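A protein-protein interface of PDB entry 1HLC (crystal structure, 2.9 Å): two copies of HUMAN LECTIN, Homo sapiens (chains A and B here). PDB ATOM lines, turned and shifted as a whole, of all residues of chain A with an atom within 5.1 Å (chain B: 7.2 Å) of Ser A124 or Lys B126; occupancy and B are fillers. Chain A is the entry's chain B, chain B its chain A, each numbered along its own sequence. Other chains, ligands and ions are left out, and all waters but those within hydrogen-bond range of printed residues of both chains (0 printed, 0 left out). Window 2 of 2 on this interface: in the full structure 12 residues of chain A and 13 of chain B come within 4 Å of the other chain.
N of Lys A16 sits at hydrogen-bond distance from O of Lys A126. O of Thr A18 sits at hydrogen-bond distance from N of Ser A123 (2.8 Å). O of Thr A18 is in hydrogen-bond range of N of Ser A124 (3.3 Å). O of Lys B126 sits at hydrogen-bond distance from N of Lys B16, 2.8 Å away. The backbone NH of Thr B18 is in hydrogen-bond range of the backbone carbonyl oxygen of Ser B124, at 2.9 Å.
The backbone carbonyl oxygen (O) of Phe A125 lies within hydrogen-bond range of the backbone NH (N) of Phe B125, 3.1 Å away. O of Ser A123 is in hydrogen-bond range of N of Leu B127, at 2.9 Å.
Of chain B, only Phe B125 (3.6 Å) and Lys B126 (3.4 Å) come within 4 Å of Ser A124. Of chain A, only Ser A123 and Ser A124 come within 4 Å of Lys B126. Of the printed residues of chain B, Phe A125 touches Ser B124 (3.1 Å) and Phe B125 (3.1 Å). Printed residues of chain B within 4 Å of Lys A126: Ser B124. Leu B15 touches none of the printed residues of chain A. The nearest printed residue of chain A that does not touch Lys B126 is Phe A125 (5.3 Å). The nearest printed residue of chain A that does not touch Phe B125 is Ser A123 (4.05 Å).
Hydrophobic or aromatic side chains of chain A that line the printed part of chain B: Phe A125. Of the 14 printed residues of chain B, 4 touch a printed residue of chain A.
Ser A124 touches Phe B125, and with the chains exchanged Phe A125 touches Ser B124. Ser A124 touches Lys B126, and with the chains exchanged Lys A126 touches Ser B124. Phe A125 touches its own counterpart, Phe B125.
Among the printed residues, pairs that only touch across the chains: Phe A125 with Ser B124 (3.1 Å), Ser A123 with Lys B126 (3.4 Å), Ser A124 with Lys B126 (3.4 Å), Lys A126 with Ser B124 (3.6 Å) and Ser A124 with Phe B125 (3.6 Å).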
ATOM      1  N   LYS A  16      -1.713  12.142 -12.793  1.00  0.00           N
ATOM      2  CA  LYS A  16      -0.557  13.027 -12.691  1.00  0.00           C
ATOM      3  C   LYS A  16      -0.509  13.975 -13.890  1.00  0.00           C
ATOM      4  O   LYS A  16      -0.025  13.655 -14.966  1.00  0.00           O
ATOM      5  CB  LYS A  16       0.724  12.212 -12.534  1.00  0.00           C
ATOM      6  CG  LYS A  16       1.878  12.965 -11.912  1.00  0.00           C
ATOM      7  CD  LYS A  16       2.526  13.919 -12.903  1.00  0.00           C
ATOM      8  CE  LYS A  16       3.796  14.556 -12.341  1.00  0.00           C
ATOM      9  NZ  LYS A  16       3.524  15.379 -11.119  1.00  0.00           N
ATOM     10  N   ILE A  17      -1.071  15.147 -13.666  1.00  0.00           N
ATOM     11  CA  ILE A  17      -1.191  16.211 -14.645  1.00  0.00           C
ATOM     12  C   ILE A  17       0.073  17.071 -14.693  1.00  0.00           C
ATOM     13  O   ILE A  17       0.770  17.223 -13.694  1.00  0.00           O
ATOM     14  CB  ILE A  17      -2.407  17.095 -14.270  1.00  0.00           C
ATOM     15  CG1 ILE A  17      -3.682  16.262 -14.306  1.00  0.00           C
ATOM     16  CG2 ILE A  17      -2.526  18.280 -15.182  1.00  0.00           C
ATOM     17  CD1 ILE A  17      -4.828  16.900 -13.571  1.00  0.00           C
ATOM     18  N   THR A  18       0.334  17.641 -15.865  1.00  0.00           N
ATOM     19  CA  THR A  18       1.478  18.519 -16.106  1.00  0.00           C
ATOM     20  C   THR A  18       1.063  19.456 -17.228  1.00  0.00           C
ATOM     21  O   THR A  18       0.304  19.055 -18.121  1.00  0.00           O
ATOM     22  CB  THR A  18       2.711  17.742 -16.580  1.00  0.00           C
ATOM     23  OG1 THR A  18       3.119  16.822 -15.562  1.00  0.00           O
ATOM     24  CG2 THR A  18       3.844  18.696 -16.904  1.00  0.00           C
ATOM     25  N   MET A 122      -2.093  21.663 -21.027  1.00  0.00           N
ATOM     26  CA  MET A 122      -1.649  20.360 -20.535  1.00  0.00           C
ATOM     27  C   MET A 122      -0.745  19.611 -21.497  1.00  0.00           C
ATOM     28  O   MET A 122      -1.053  19.483 -22.676  1.00  0.00           O
ATOM     29  CB  MET A 122      -2.849  19.491 -20.208  1.00  0.00           C
ATOM     30  CG  MET A 122      -2.489  18.062 -19.886  1.00  0.00           C
ATOM     31  SD  MET A 122      -3.927  17.001 -19.958  1.00  0.00           S
ATOM     32  CE  MET A 122      -4.591  17.199 -18.268  1.00  0.00           C
ATOM     33  N   SER A 123       0.320  19.040 -20.951  1.00  0.00           N
ATOM     34  CA  SER A 123       1.307  18.318 -21.726  1.00  0.00           C
ATOM     35  C   SER A 123       1.427  16.854 -21.344  1.00  0.00           C
ATOM     36  O   SER A 123       1.933  16.054 -22.119  1.00  0.00           O
ATOM     37  CB  SER A 123       2.674  19.008 -21.593  1.00  0.00           C
ATOM     38  OG  SER A 123       3.065  19.179 -20.225  1.00  0.00           O
ATOM     39  N   SER A 124       1.024  16.509 -20.129  1.00  0.00           N
ATOM     40  CA  SER A 124       1.092  15.124 -19.686  1.00  0.00           C
ATOM     41  C   SER A 124      -0.143  14.705 -18.950  1.00  0.00           C
ATOM     42  O   SER A 124      -0.880  15.523 -18.421  1.00  0.00           O
ATOM     43  CB  SER A 124       2.301  14.864 -18.802  1.00  0.00           C
ATOM     44  OG  SER A 124       3.441  14.630 -19.591  1.00  0.00           O
ATOM     45  N   PHE A 125      -0.326  13.405 -18.899  1.00  0.00           N
ATOM     46  CA  PHE A 125      -1.452  12.789 -18.255  1.00  0.00           C
ATOM     47  C   PHE A 125      -0.935  11.384 -18.043  1.00  0.00           C
ATOM     48  O   PHE A 125      -0.423  10.767 -18.975  1.00  0.00           O
ATOM     49  CB  PHE A 125      -2.634  12.791 -19.219  1.00  0.00           C
ATOM     50  CG  PHE A 125      -3.756  11.877 -18.830  1.00  0.00           C
ATOM     51  CD1 PHE A 125      -3.715  10.517 -19.156  1.00  0.00           C
ATOM     52  CD2 PHE A 125      -4.897  12.377 -18.216  1.00  0.00           C
ATOM     53  CE1 PHE A 125      -4.798   9.664 -18.884  1.00  0.00           C
ATOM     54  CE2 PHE A 125      -5.981  11.537 -17.941  1.00  0.00           C
ATOM     55  CZ  PHE A 125      -5.927  10.172 -18.282  1.00  0.00           C
ATOM     56  N   LYS A 126      -0.926  10.946 -16.795  1.00  0.00           N
ATOM     57  CA  LYS A 126      -0.487   9.608 -16.463  1.00  0.00           C
ATOM     58  C   LYS A 126      -1.477   9.117 -15.441  1.00  0.00           C
ATOM     59  O   LYS A 126      -1.842   9.844 -14.520  1.00  0.00           O
ATOM     60  CB  LYS A 126       0.919   9.605 -15.870  1.00  0.00           C
ATOM     61  CG  LYS A 126       1.501   8.198 -15.671  1.00  0.00           C
ATOM     62  CD  LYS A 126       2.889   8.265 -15.029  1.00  0.00           C
ATOM     63  CE  LYS A 126       3.463   6.879 -14.786  1.00  0.00           C
ATOM     64  NZ  LYS A 126       4.717   6.889 -13.974  1.00  0.00           N
ATOM     65  N   THR B  14       5.062  16.101 -31.119  1.00  0.00           N
ATOM     66  CA  THR B  14       5.149  14.663 -31.059  1.00  0.00           C
ATOM     67  C   THR B  14       4.242  14.194 -29.933  1.00  0.00           C
ATOM     68  O   THR B  14       4.235  14.771 -28.853  1.00  0.00           O
ATOM     69  CB  THR B  14       6.609  14.233 -30.808  1.00  0.00           C
ATOM     70  OG1 THR B  14       7.481  14.950 -31.696  1.00  0.00           O
ATOM     71  CG2 THR B  14       6.789  12.751 -31.060  1.00  0.00           C
ATOM     72  N   LEU B  15       3.428  13.189 -30.216  1.00  0.00           N
ATOM     73  CA  LEU B  15       2.513  12.636 -29.235  1.00  0.00           C
ATOM     74  C   LEU B  15       3.047  11.276 -28.838  1.00  0.00           C
ATOM     75  O   LEU B  15       3.259  10.428 -29.691  1.00  0.00           O
ATOM     76  CB  LEU B  15       1.139  12.481 -29.854  1.00  0.00           C
ATOM     77  CG  LEU B  15       0.058  11.974 -28.912  1.00  0.00           C
ATOM     78  CD1 LEU B  15      -0.381  13.108 -27.967  1.00  0.00           C
ATOM     79  CD2 LEU B  15      -1.104  11.470 -29.750  1.00  0.00           C
ATOM     80  N   LYS B  16       3.268  11.074 -27.549  1.00  0.00           N
ATOM     81  CA  LYS B  16       3.808   9.822 -27.041  1.00  0.00           C
ATOM     82  C   LYS B  16       2.741   9.069 -26.240  1.00  0.00           C
ATOM     83  O   LYS B  16       2.390   9.459 -25.130  1.00  0.00           O
ATOM     84  CB  LYS B  16       5.038  10.124 -26.180  1.00  0.00           C
ATOM     85  CG  LYS B  16       5.674   8.903 -25.566  1.00  0.00           C
ATOM     86  CD  LYS B  16       6.336   8.061 -26.641  1.00  0.00           C
ATOM     87  CE  LYS B  16       6.850   6.735 -26.106  1.00  0.00           C
ATOM     88  NZ  LYS B  16       7.770   6.856 -24.919  1.00  0.00           N
ATOM     89  N   ILE B  17       2.263   7.964 -26.793  1.00  0.00           N
ATOM     90  CA  ILE B  17       1.207   7.185 -26.175  1.00  0.00           C
ATOM     91  C   ILE B  17       1.669   5.859 -25.595  1.00  0.00           C
ATOM     92  O   ILE B  17       2.161   5.006 -26.313  1.00  0.00           O
ATOM     93  CB  ILE B  17       0.088   6.926 -27.203  1.00  0.00           C
ATOM     94  CG1 ILE B  17      -0.625   8.239 -27.545  1.00  0.00           C
ATOM     95  CG2 ILE B  17      -0.912   5.902 -26.678  1.00  0.00           C
ATOM     96  CD1 ILE B  17      -1.543   8.139 -28.726  1.00  0.00           C
ATOM     97  N   THR B  18       1.486   5.671 -24.299  1.00  0.00           N
ATOM     98  CA  THR B  18       1.877   4.422 -23.660  1.00  0.00           C
ATOM     99  C   THR B  18       0.613   3.775 -23.144  1.00  0.00           C
ATOM    100  O   THR B  18      -0.220   4.443 -22.537  1.00  0.00           O
ATOM    101  CB  THR B  18       2.887   4.659 -22.487  1.00  0.00           C
ATOM    102  OG1 THR B  18       4.126   5.142 -23.016  1.00  0.00           O
ATOM    103  CG2 THR B  18       3.160   3.372 -21.698  1.00  0.00           C
ATOM    104  N   THR B  82       4.989   6.471 -30.733  1.00  0.00           N
ATOM    105  CA  THR B  82       5.295   7.886 -30.806  1.00  0.00           C
ATOM    106  C   THR B  82       4.926   8.348 -32.203  1.00  0.00           C
ATOM    107  O   THR B  82       5.571   7.957 -33.168  1.00  0.00           O
ATOM    108  CB  THR B  82       6.775   8.162 -30.552  1.00  0.00           C
ATOM    109  OG1 THR B  82       7.237   7.340 -29.474  1.00  0.00           O
ATOM    110  CG2 THR B  82       6.982   9.615 -30.184  1.00  0.00           C
ATOM    111  N   VAL B  83       3.814   9.065 -32.326  1.00  0.00           N
ATOM    112  CA  VAL B  83       3.404   9.584 -33.626  1.00  0.00           C
ATOM    113  C   VAL B  83       3.650  11.090 -33.660  1.00  0.00           C
ATOM    114  O   VAL B  83       3.281  11.825 -32.744  1.00  0.00           O
ATOM    115  CB  VAL B  83       1.927   9.202 -34.030  1.00  0.00           C
ATOM    116  CG1 VAL B  83       1.072   8.924 -32.813  1.00  0.00           C
ATOM    117  CG2 VAL B  83       1.297  10.295 -34.907  1.00  0.00           C
ATOM    118  N   MET B 122      -4.718   2.881 -22.561  1.00  0.00           N
ATOM    119  CA  MET B 122      -3.550   3.739 -22.364  1.00  0.00           C
ATOM    120  C   MET B 122      -3.418   4.405 -21.017  1.00  0.00           C
ATOM    121  O   MET B 122      -4.273   5.174 -20.600  1.00  0.00           O
ATOM    122  CB  MET B 122      -3.332   4.756 -23.500  1.00  0.00           C
ATOM    123  CG  MET B 122      -4.459   5.681 -23.787  1.00  0.00           C
ATOM    124  SD  MET B 122      -3.835   7.269 -24.278  1.00  0.00           S
ATOM    125  CE  MET B 122      -3.944   8.120 -22.710  1.00  0.00           C
ATOM    126  N   SER B 124      -0.947   6.540 -20.216  1.00  0.00           N
ATOM    127  CA  SER B 124      -0.460   7.902 -20.270  1.00  0.00           C
ATOM    128  C   SER B 124      -0.137   8.391 -21.659  1.00  0.00           C
ATOM    129  O   SER B 124       0.265   7.598 -22.505  1.00  0.00           O
ATOM    130  CB  SER B 124       0.814   7.997 -19.432  1.00  0.00           C
ATOM    131  OG  SER B 124       1.832   7.156 -19.957  1.00  0.00           O
ATOM    132  N   PHE B 125      -0.286   9.694 -21.876  1.00  0.00           N
ATOM    133  CA  PHE B 125       0.071  10.301 -23.147  1.00  0.00           C
ATOM    134  C   PHE B 125       0.843  11.581 -22.854  1.00  0.00           C
ATOM    135  O   PHE B 125       0.574  12.252 -21.869  1.00  0.00           O
ATOM    136  CB  PHE B 125      -1.138  10.506 -24.089  1.00  0.00           C
ATOM    137  CG  PHE B 125      -2.077  11.608 -23.690  1.00  0.00           C
ATOM    138  CD1 PHE B 125      -3.104  11.373 -22.773  1.00  0.00           C
ATOM    139  CD2 PHE B 125      -1.968  12.871 -24.274  1.00  0.00           C
ATOM    140  CE1 PHE B 125      -4.011  12.369 -22.439  1.00  0.00           C
ATOM    141  CE2 PHE B 125      -2.870  13.890 -23.953  1.00  0.00           C
ATOM    142  CZ  PHE B 125      -3.900  13.636 -23.027  1.00  0.00           C
ATOM    143  N   LYS B 126       1.819  11.895 -23.693  1.00  0.00           N
ATOM    144  CA  LYS B 126       2.671  13.057 -23.492  1.00  0.00           C
ATOM    145  C   LYS B 126       2.813  13.831 -24.801  1.00  0.00           C
ATOM    146  O   LYS B 126       3.254  13.282 -25.805  1.00  0.00           O
ATOM    147  CB  LYS B 126       4.031  12.537 -23.014  1.00  0.00           C
ATOM    148  CG  LYS B 126       5.012  13.533 -22.424  1.00  0.00           C
ATOM    149  CD  LYS B 126       5.660  14.432 -23.468  1.00  0.00           C
ATOM    150  CE  LYS B 126       6.860  15.186 -22.889  1.00  0.00           C
ATOM    151  NZ  LYS B 126       7.976  14.248 -22.532  1.00  0.00           N
ATOM    152  N   LEU B 127       2.446  15.109 -24.790  1.00  0.00           N
ATOM    153  CA  LEU B 127       2.541  15.928 -25.991  1.00  0.00           C
ATOM    154  C   LEU B 127       3.787  16.791 -26.000  1.00  0.00           C
ATOM    155  O   LEU B 127       3.841  17.801 -25.315  1.00  0.00           O
ATOM    156  CB  LEU B 127       1.304  16.816 -26.145  1.00  0.00           C
ATOM    157  CG  LEU B 127       0.556  16.616 -27.471  1.00  0.00           C
ATOM    158  CD1 LEU B 127      -0.603  17.575 -27.591  1.00  0.00           C
ATOM    159  CD2 LEU B 127       1.503  16.799 -28.644  1.00  0.00           C
ATOM    160  N   LYS B 128       4.791  16.394 -26.775  1.00  0.00           N
ATOM    161  CA  LYS B 128       6.040  17.155 -26.872  1.00  0.00           C
ATOM    162  C   LYS B 128       5.932  18.279 -27.898  1.00  0.00           C
ATOM    163  O   LYS B 128       5.089  18.244 -28.796  1.00  0.00           O
ATOM    164  CB  LYS B 128       7.218  16.248 -27.267  1.00  0.00           C
ATOM    165  CG  LYS B 128       7.543  15.071 -26.322  1.00  0.00           C
ATOM    166  CD  LYS B 128       6.721  13.808 -26.640  1.00  0.00           C
ATOM    167  CE  LYS B 128       7.422  12.513 -26.196  1.00  0.00           C
ATOM    168  NZ  LYS B 128       7.544  12.323 -24.717  1.00  0.00           N
ATOM    169  N   GLU B 129       6.784  19.285 -27.759  1.00  0.00           N
ATOM    170  CA  GLU B 129       6.794  20.401 -28.704  1.00  0.00           C
ATOM    171  C   GLU B 129       7.662  19.963 -29.905  1.00  0.00           C
ATOM    172  O   GLU B 129       7.744  20.713 -30.917  1.00  0.00           O
ATOM    173  CB  GLU B 129       7.375  21.671 -28.048  1.00  0.00           C
ATOM    174  CG  GLU B 129       6.896  23.001 -28.694  1.00  0.00           C
ATOM    175  CD  GLU B 129       7.623  24.266 -28.169  1.00  0.00           C
ATOM    176  OE1 GLU B 129       7.169  24.844 -27.135  1.00  0.00           O
ATOM    177  OE2 GLU B 129       8.626  24.693 -28.818  1.00  0.00           O
ATOM    178  OXT GLU B 129       8.240  18.844 -29.821  1.00  0.00           O
